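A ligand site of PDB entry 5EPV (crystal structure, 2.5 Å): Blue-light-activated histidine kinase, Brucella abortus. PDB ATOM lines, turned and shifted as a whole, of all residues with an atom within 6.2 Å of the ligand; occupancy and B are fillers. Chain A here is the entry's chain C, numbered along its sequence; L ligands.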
ATOM      1  N   GLU A 122      10.034 -37.441 -17.554  1.00  0.00           N
ATOM      2  CA  GLU A 122       9.633 -36.050 -17.683  1.00  0.00           C
ATOM      3  C   GLU A 122       9.411 -35.690 -19.171  1.00  0.00           C
ATOM      4  O   GLU A 122       8.466 -34.977 -19.478  1.00  0.00           O
ATOM      5  CB  GLU A 122      10.699 -35.163 -17.033  1.00  0.00           C
ATOM      6  CG  GLU A 122      10.206 -33.806 -16.596  1.00  0.00           C
ATOM      7  CD  GLU A 122       8.982 -33.757 -15.685  1.00  0.00           C
ATOM      8  OE1 GLU A 122       8.226 -32.756 -15.792  1.00  0.00           O
ATOM      9  OE2 GLU A 122       8.807 -34.665 -14.843  1.00  0.00           O
ATOM     10  N   LEU A 123      10.276 -36.199 -20.058  1.00  0.00           N
ATOM     11  CA  LEU A 123      10.190 -35.935 -21.491  1.00  0.00           C
ATOM     12  C   LEU A 123       8.979 -36.592 -22.120  1.00  0.00           C
ATOM     13  O   LEU A 123       8.322 -35.976 -22.950  1.00  0.00           O
ATOM     14  CB  LEU A 123      11.481 -36.315 -22.232  1.00  0.00           C
ATOM     15  CG  LEU A 123      12.729 -35.504 -21.849  1.00  0.00           C
ATOM     16  CD1 LEU A 123      14.002 -36.201 -22.299  1.00  0.00           C
ATOM     17  CD2 LEU A 123      12.620 -34.058 -22.279  1.00  0.00           C
ATOM     18  N   ASN A 126       5.774 -34.671 -21.095  1.00  0.00           N
ATOM     19  CA  ASN A 126       5.555 -33.536 -21.985  1.00  0.00           C
ATOM     20  C   ASN A 126       5.181 -33.947 -23.407  1.00  0.00           C
ATOM     21  O   ASN A 126       4.407 -33.245 -24.049  1.00  0.00           O
ATOM     22  CB  ASN A 126       6.747 -32.600 -21.953  1.00  0.00           C
ATOM     23  CG  ASN A 126       6.930 -31.942 -20.627  1.00  0.00           C
ATOM     24  OD1 ASN A 126       5.992 -31.802 -19.844  1.00  0.00           O
ATOM     25  ND2 ASN A 126       8.155 -31.529 -20.325  1.00  0.00           N
ATOM     26  N   ALA A 127       5.710 -35.076 -23.906  1.00  0.00           N
ATOM     27  CA  ALA A 127       5.419 -35.598 -25.245  1.00  0.00           C
ATOM     28  C   ALA A 127       3.901 -35.841 -25.432  1.00  0.00           C
ATOM     29  O   ALA A 127       3.356 -35.569 -26.503  1.00  0.00           O
ATOM     30  CB  ALA A 127       6.187 -36.872 -25.491  1.00  0.00           C
ATOM     31  N   TYR A 130       2.309 -31.973 -25.041  1.00  0.00           N
ATOM     32  CA  TYR A 130       2.594 -31.036 -26.141  1.00  0.00           C
ATOM     33  C   TYR A 130       3.133 -31.601 -27.473  1.00  0.00           C
ATOM     34  O   TYR A 130       2.883 -30.990 -28.506  1.00  0.00           O
ATOM     35  CB  TYR A 130       3.567 -29.950 -25.668  1.00  0.00           C
ATOM     36  CG  TYR A 130       3.323 -29.368 -24.292  1.00  0.00           C
ATOM     37  CD1 TYR A 130       2.308 -28.453 -24.060  1.00  0.00           C
ATOM     38  CD2 TYR A 130       4.185 -29.667 -23.234  1.00  0.00           C
ATOM     39  CE1 TYR A 130       2.105 -27.889 -22.795  1.00  0.00           C
ATOM     40  CE2 TYR A 130       4.003 -29.100 -21.974  1.00  0.00           C
ATOM     41  CZ  TYR A 130       2.964 -28.216 -21.762  1.00  0.00           C
ATOM     42  OH  TYR A 130       2.813 -27.656 -20.514  1.00  0.00           O
ATOM     43  N   GLY A 131       3.907 -32.678 -27.422  1.00  0.00           N
ATOM     44  CA  GLY A 131       4.617 -33.205 -28.583  1.00  0.00           C
ATOM     45  C   GLY A 131       4.081 -34.444 -29.262  1.00  0.00           C
ATOM     46  O   GLY A 131       2.865 -34.620 -29.384  1.00  0.00           O
ATOM     47  N   ALA A 132       5.024 -35.293 -29.730  1.00  0.00           N
ATOM     48  CA  ALA A 132       4.764 -36.528 -30.467  1.00  0.00           C
ATOM     49  C   ALA A 132       3.675 -37.476 -29.911  1.00  0.00           C
ATOM     50  O   ALA A 132       3.089 -38.218 -30.679  1.00  0.00           O
ATOM     51  CB  ALA A 132       6.068 -37.282 -30.698  1.00  0.00           C
ATOM     52  N   TRP A 159      17.073 -37.807 -28.075  1.00  0.00           N
ATOM     53  CA  TRP A 159      15.641 -37.947 -27.852  1.00  0.00           C
ATOM     54  C   TRP A 159      15.092 -37.125 -29.009  1.00  0.00           C
ATOM     55  O   TRP A 159      15.284 -35.921 -29.046  1.00  0.00           O
ATOM     56  CB  TRP A 159      15.198 -37.357 -26.494  1.00  0.00           C
ATOM     57  CG  TRP A 159      13.687 -37.297 -26.318  1.00  0.00           C
ATOM     58  CD1 TRP A 159      12.835 -36.396 -26.878  1.00  0.00           C
ATOM     59  CD2 TRP A 159      12.878 -38.157 -25.498  1.00  0.00           C
ATOM     60  NE1 TRP A 159      11.544 -36.681 -26.489  1.00  0.00           N
ATOM     61  CE2 TRP A 159      11.542 -37.738 -25.636  1.00  0.00           C
ATOM     62  CE3 TRP A 159      13.164 -39.243 -24.662  1.00  0.00           C
ATOM     63  CZ2 TRP A 159      10.477 -38.372 -24.964  1.00  0.00           C
ATOM     64  CZ3 TRP A 159      12.120 -39.855 -23.993  1.00  0.00           C
ATOM     65  CH2 TRP A 159      10.796 -39.415 -24.128  1.00  0.00           C
ATOM     66  N   GLU A 161      11.602 -36.335 -31.318  1.00  0.00           N
ATOM     67  CA  GLU A 161      10.152 -36.359 -31.543  1.00  0.00           C
ATOM     68  C   GLU A 161       9.873 -35.936 -32.995  1.00  0.00           C
ATOM     69  O   GLU A 161      10.391 -34.916 -33.444  1.00  0.00           O
ATOM     70  CB  GLU A 161       9.429 -35.404 -30.579  1.00  0.00           C
ATOM     71  CG  GLU A 161       9.769 -35.662 -29.121  1.00  0.00           C
ATOM     72  CD  GLU A 161       8.899 -34.943 -28.108  1.00  0.00           C
ATOM     73  OE1 GLU A 161       9.381 -34.773 -26.960  1.00  0.00           O
ATOM     74  OE2 GLU A 161       7.750 -34.574 -28.438  1.00  0.00           O
ATOM     75  N   GLU A 166       2.893 -29.065 -34.702  1.00  0.00           N
ATOM     76  CA  GLU A 166       3.896 -28.033 -34.887  1.00  0.00           C
ATOM     77  C   GLU A 166       4.349 -27.520 -33.540  1.00  0.00           C
ATOM     78  O   GLU A 166       3.523 -27.321 -32.641  1.00  0.00           O
ATOM     79  CB  GLU A 166       3.382 -26.870 -35.768  1.00  0.00           C
ATOM     80  CG  GLU A 166       4.222 -26.596 -37.015  1.00  0.00           C
ATOM     81  CD  GLU A 166       4.917 -25.257 -37.161  1.00  0.00           C
ATOM     82  OE1 GLU A 166       5.050 -24.516 -36.153  1.00  0.00           O
ATOM     83  OE2 GLU A 166       5.372 -24.950 -38.286  1.00  0.00           O
ATOM     84  N   VAL A 167       5.667 -27.319 -33.384  1.00  0.00           N
ATOM     85  CA  VAL A 167       6.165 -26.795 -32.124  1.00  0.00           C
ATOM     86  C   VAL A 167       6.314 -25.278 -32.208  1.00  0.00           C
ATOM     87  O   VAL A 167       7.256 -24.739 -32.808  1.00  0.00           O
ATOM     88  CB  VAL A 167       7.185 -27.646 -31.301  1.00  0.00           C
ATOM     89  CG1 VAL A 167       7.428 -29.016 -31.921  1.00  0.00           C
ATOM     90  CG2 VAL A 167       8.483 -26.936 -30.986  1.00  0.00           C
ATOM     91  N   MET A 168       5.253 -24.609 -31.725  1.00  0.00           N
ATOM     92  CA  MET A 168       5.013 -23.168 -31.712  1.00  0.00           C
ATOM     93  C   MET A 168       6.086 -22.334 -31.030  1.00  0.00           C
ATOM     94  O   MET A 168       6.355 -22.495 -29.834  1.00  0.00           O
ATOM     95  CB  MET A 168       3.588 -22.847 -31.225  1.00  0.00           C
ATOM     96  CG  MET A 168       2.601 -22.581 -32.362  1.00  0.00           C
ATOM     97  SD  MET A 168       2.608 -23.761 -33.766  1.00  0.00           S
ATOM     98  CE  MET A 168       1.232 -23.135 -34.731  1.00  0.00           C
ATOM     99  N   PRO A 170       7.180 -19.547 -29.257  1.00  0.00           N
ATOM    100  CA  PRO A 170       7.555 -19.224 -27.864  1.00  0.00           C
ATOM    101  C   PRO A 170       7.651 -20.397 -26.862  1.00  0.00           C
ATOM    102  O   PRO A 170       7.385 -20.205 -25.658  1.00  0.00           O
ATOM    103  CB  PRO A 170       6.541 -18.143 -27.461  1.00  0.00           C
ATOM    104  CG  PRO A 170       5.354 -18.421 -28.267  1.00  0.00           C
ATOM    105  CD  PRO A 170       5.814 -19.055 -29.563  1.00  0.00           C
ATOM    106  N   ALA A 171       8.067 -21.596 -27.335  1.00  0.00           N
ATOM    107  CA  ALA A 171       8.256 -22.761 -26.473  1.00  0.00           C
ATOM    108  C   ALA A 171       9.555 -22.586 -25.657  1.00  0.00           C
ATOM    109  O   ALA A 171      10.656 -22.786 -26.187  1.00  0.00           O
ATOM    110  CB  ALA A 171       8.294 -24.048 -27.299  1.00  0.00           C
ATOM    111  N   ARG A 172       9.424 -22.126 -24.402  1.00  0.00           N
ATOM    112  CA  ARG A 172      10.538 -21.871 -23.497  1.00  0.00           C
ATOM    113  C   ARG A 172      10.348 -22.591 -22.147  1.00  0.00           C
ATOM    114  O   ARG A 172       9.336 -22.368 -21.457  1.00  0.00           O
ATOM    115  CB  ARG A 172      10.714 -20.368 -23.280  1.00  0.00           C
ATOM    116  N   ARG A 173      11.342 -23.454 -21.805  1.00  0.00           N
ATOM    117  CA  ARG A 173      11.425 -24.303 -20.604  1.00  0.00           C
ATOM    118  C   ARG A 173      11.241 -23.539 -19.297  1.00  0.00           C
ATOM    119  O   ARG A 173      11.749 -22.427 -19.168  1.00  0.00           O
ATOM    120  CB  ARG A 173      12.776 -25.036 -20.550  1.00  0.00           C
ATOM    121  CG  ARG A 173      13.027 -26.053 -21.658  1.00  0.00           C
ATOM    122  CD  ARG A 173      14.417 -26.665 -21.583  1.00  0.00           C
ATOM    123  NE  ARG A 173      15.459 -25.646 -21.451  1.00  0.00           N
ATOM    124  CZ  ARG A 173      16.706 -25.894 -21.043  1.00  0.00           C
ATOM    125  NH1 ARG A 173      17.087 -27.128 -20.753  1.00  0.00           N
ATOM    126  NH2 ARG A 173      17.572 -24.897 -20.924  1.00  0.00           N
ATOM    127  N   GLY A 174      10.531 -24.161 -18.347  1.00  0.00           N
ATOM    128  CA  GLY A 174      10.330 -23.655 -16.994  1.00  0.00           C
ATOM    129  C   GLY A 174      11.458 -24.161 -16.107  1.00  0.00           C
ATOM    130  O   GLY A 174      12.323 -24.916 -16.575  1.00  0.00           O
ATOM    131  N   PHE A 175      11.469 -23.754 -14.828  1.00  0.00           N
ATOM    132  CA  PHE A 175      12.512 -24.162 -13.869  1.00  0.00           C
ATOM    133  C   PHE A 175      12.808 -25.669 -13.762  1.00  0.00           C
ATOM    134  O   PHE A 175      13.986 -26.048 -13.765  1.00  0.00           O
ATOM    135  CB  PHE A 175      12.274 -23.559 -12.497  1.00  0.00           C
ATOM    136  CG  PHE A 175      13.432 -23.747 -11.550  1.00  0.00           C
ATOM    137  CD1 PHE A 175      14.609 -23.026 -11.718  1.00  0.00           C
ATOM    138  CD2 PHE A 175      13.338 -24.618 -10.475  1.00  0.00           C
ATOM    139  CE1 PHE A 175      15.684 -23.165 -10.817  1.00  0.00           C
ATOM    140  CE2 PHE A 175      14.406 -24.758  -9.568  1.00  0.00           C
ATOM    141  CZ  PHE A 175      15.577 -24.036  -9.758  1.00  0.00           C
ATOM    142  N   GLY A 176      11.750 -26.477 -13.655  1.00  0.00           N
ATOM    143  CA  GLY A 176      11.823 -27.924 -13.493  1.00  0.00           C
ATOM    144  C   GLY A 176      12.640 -28.666 -14.527  1.00  0.00           C
ATOM    145  O   GLY A 176      13.641 -29.297 -14.185  1.00  0.00           O
ATOM    146  N   GLN A 177      12.206 -28.591 -15.798  1.00  0.00           N
ATOM    147  CA  GLN A 177      12.884 -29.212 -16.935  1.00  0.00           C
ATOM    148  C   GLN A 177      14.301 -28.670 -17.045  1.00  0.00           C
ATOM    149  O   GLN A 177      15.238 -29.460 -17.159  1.00  0.00           O
ATOM    150  CB  GLN A 177      12.102 -28.988 -18.241  1.00  0.00           C
ATOM    151  N   ARG A 178      14.472 -27.354 -16.881  1.00  0.00           N
ATOM    152  CA  ARG A 178      15.789 -26.715 -16.906  1.00  0.00           C
ATOM    153  C   ARG A 178      16.692 -27.391 -15.879  1.00  0.00           C
ATOM    154  O   ARG A 178      17.788 -27.838 -16.217  1.00  0.00           O
ATOM    155  CB  ARG A 178      15.634 -25.224 -16.587  1.00  0.00           C
ATOM    156  CG  ARG A 178      16.779 -24.347 -17.086  1.00  0.00           C
ATOM    157  CD  ARG A 178      16.611 -22.845 -16.782  1.00  0.00           C
ATOM    158  NE  ARG A 178      15.413 -22.302 -17.430  1.00  0.00           N
ATOM    159  CZ  ARG A 178      14.277 -22.085 -16.781  1.00  0.00           C
ATOM    160  NH1 ARG A 178      14.196 -22.289 -15.481  1.00  0.00           N
ATOM    161  NH2 ARG A 178      13.227 -21.612 -17.435  1.00  0.00           N
ATOM    162  N   PHE A 196      13.817 -26.916 -29.827  1.00  0.00           N
ATOM    163  CA  PHE A 196      12.369 -26.934 -30.001  1.00  0.00           C
ATOM    164  C   PHE A 196      12.019 -26.694 -31.491  1.00  0.00           C
ATOM    165  O   PHE A 196      11.263 -25.785 -31.819  1.00  0.00           O
ATOM    166  CB  PHE A 196      11.704 -25.900 -29.096  1.00  0.00           C
ATOM    167  CG  PHE A 196      11.812 -26.215 -27.630  1.00  0.00           C
ATOM    168  CD1 PHE A 196      10.764 -26.857 -26.971  1.00  0.00           C
ATOM    169  CD2 PHE A 196      12.928 -25.825 -26.892  1.00  0.00           C
ATOM    170  CE1 PHE A 196      10.850 -27.126 -25.603  1.00  0.00           C
ATOM    171  CE2 PHE A 196      13.008 -26.094 -25.531  1.00  0.00           C
ATOM    172  CZ  PHE A 196      11.970 -26.744 -24.894  1.00  0.00           C
ATOM    173  N   GLY A 200       9.516 -31.152 -34.325  1.00  0.00           N
ATOM    174  CA  GLY A 200       9.522 -31.890 -33.071  1.00  0.00           C
ATOM    175  C   GLY A 200      10.733 -31.625 -32.206  1.00  0.00           C
ATOM    176  O   GLY A 200      11.822 -31.303 -32.726  1.00  0.00           O
ATOM    177  N   LEU A 201      10.543 -31.729 -30.879  1.00  0.00           N
ATOM    178  CA  LEU A 201      11.618 -31.543 -29.892  1.00  0.00           C
ATOM    179  C   LEU A 201      12.751 -32.541 -30.119  1.00  0.00           C
ATOM    180  O   LEU A 201      12.495 -33.719 -30.315  1.00  0.00           O
ATOM    181  CB  LEU A 201      11.074 -31.641 -28.457  1.00  0.00           C
ATOM    182  CG  LEU A 201      12.094 -31.533 -27.311  1.00  0.00           C
ATOM    183  CD1 LEU A 201      12.554 -30.120 -27.095  1.00  0.00           C
ATOM    184  CD2 LEU A 201      11.527 -32.080 -26.061  1.00  0.00           C
HETATM  185  P1  LIG L   1       4.762 -27.807 -16.802  1.00  0.00           P
HETATM  186  O1  LIG L   1       5.051 -29.042 -17.677  1.00  0.00           O
HETATM  187  O2  LIG L   1       3.344 -27.986 -16.217  1.00  0.00           O
HETATM  188  O3  LIG L   1       5.798 -27.580 -15.744  1.00  0.00           O
HETATM  189  P2  LIG L   1       5.966 -25.215 -17.797  1.00  0.00           P
HETATM  190  O4  LIG L   1       5.716 -24.051 -18.815  1.00  0.00           O
HETATM  191  O5  LIG L   1       6.508 -24.777 -16.433  1.00  0.00           O
HETATM  192  C1  LIG L   1       4.686 -26.396 -17.866  1.00  0.00           C
HETATM  193  P3  LIG L   1       7.800 -26.950 -19.312  1.00  0.00           P
HETATM  194  O6  LIG L   1       7.253 -28.307 -19.068  1.00  0.00           O
HETATM  195  O7  LIG L   1       9.303 -26.795 -19.541  1.00  0.00           O
HETATM  196  O8  LIG L   1       7.369 -25.773 -18.350  1.00  0.00           O
HETATM  197  O9  LIG L   1       7.345 -26.517 -20.802  1.00  0.00           O
HETATM  198  C2  LIG L   1       7.462 -25.212 -21.393  1.00  0.00           C
HETATM  199  C3  LIG L   1       6.818 -25.285 -22.755  1.00  0.00           C
HETATM  200  O10 LIG L   1       7.630 -26.090 -23.632  1.00  0.00           O
HETATM  201  C4  LIG L   1       5.453 -25.952 -22.794  1.00  0.00           C
HETATM  202  O11 LIG L   1       4.394 -25.096 -22.373  1.00  0.00           O
HETATM  203  C5  LIG L   1       5.340 -26.351 -24.261  1.00  0.00           C
HETATM  204  O12 LIG L   1       4.852 -25.282 -25.062  1.00  0.00           O
HETATM  205  C6  LIG L   1       6.794 -26.681 -24.617  1.00  0.00           C
HETATM  206  N1  LIG L   1       7.073 -28.111 -24.726  1.00  0.00           N
HETATM  207  C7  LIG L   1       7.585 -28.939 -23.758  1.00  0.00           C
HETATM  208  N2  LIG L   1       7.768 -30.181 -24.159  1.00  0.00           N
HETATM  209  C8  LIG L   1       7.365 -30.160 -25.481  1.00  0.00           C
HETATM  210  C9  LIG L   1       7.333 -31.155 -26.487  1.00  0.00           C
HETATM  211  N3  LIG L   1       7.703 -32.423 -26.280  1.00  0.00           N
HETATM  212  N4  LIG L   1       6.876 -30.804 -27.707  1.00  0.00           N
HETATM  213  C10 LIG L   1       6.463 -29.549 -27.906  1.00  0.00           C
HETATM  214  N5  LIG L   1       6.429 -28.527 -27.039  1.00  0.00           N
HETATM  215  C11 LIG L   1       6.911 -28.894 -25.840  1.00  0.00           C
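N of Gly 174 lies within hydrogen-bond range of O7 of the ligand, 3.1 Å away. The side-chain carboxylate of Glu 161 is in hydrogen-bond range of a nitrogen (N3) of the ligand (3.0 Å).
OE2 of Glu 161 sits at hydrogen-bond distance from N of Ala 132 (3.1 Å). The backbone carbonyl oxygen (O) of Arg 173 lies within hydrogen-bond range of the guanidinium group (NH2) of Arg 178. The backbone NH (N) of Gly 131 is in hydrogen-bond range of the backbone carbonyl oxygen (O) of Asn 126, 3.5 Å away. The backbone NH (N) of Glu 161 lies within hydrogen-bond range of the backbone carbonyl oxygen (O) of Leu 201 (2.9 Å). The guanidinium group (NH1) of Arg 178 sits close to the backbone carbonyl oxygen (O) of Gly 174 (3.4 Å). NE1 of Trp 159 is in hydrogen-bond range of OE1 of Glu 161 (2.9 Å).
Residues that only touch the ligand: Arg 172 (3.4 Å), Gly 131 (3.4 Å), Asn 126 (3.4 Å), Arg 173 (3.4 Å), Tyr 130 (3.5 Å), Gln 177 (3.8 Å), Leu 201 (3.8 Å), Phe 196 (3.9 Å) and Val 167 (3.96 Å). Hydrophobic or aromatic side chains within 4 Å of the ligand: Tyr 130, Val 167, Phe 196 and Leu 201.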
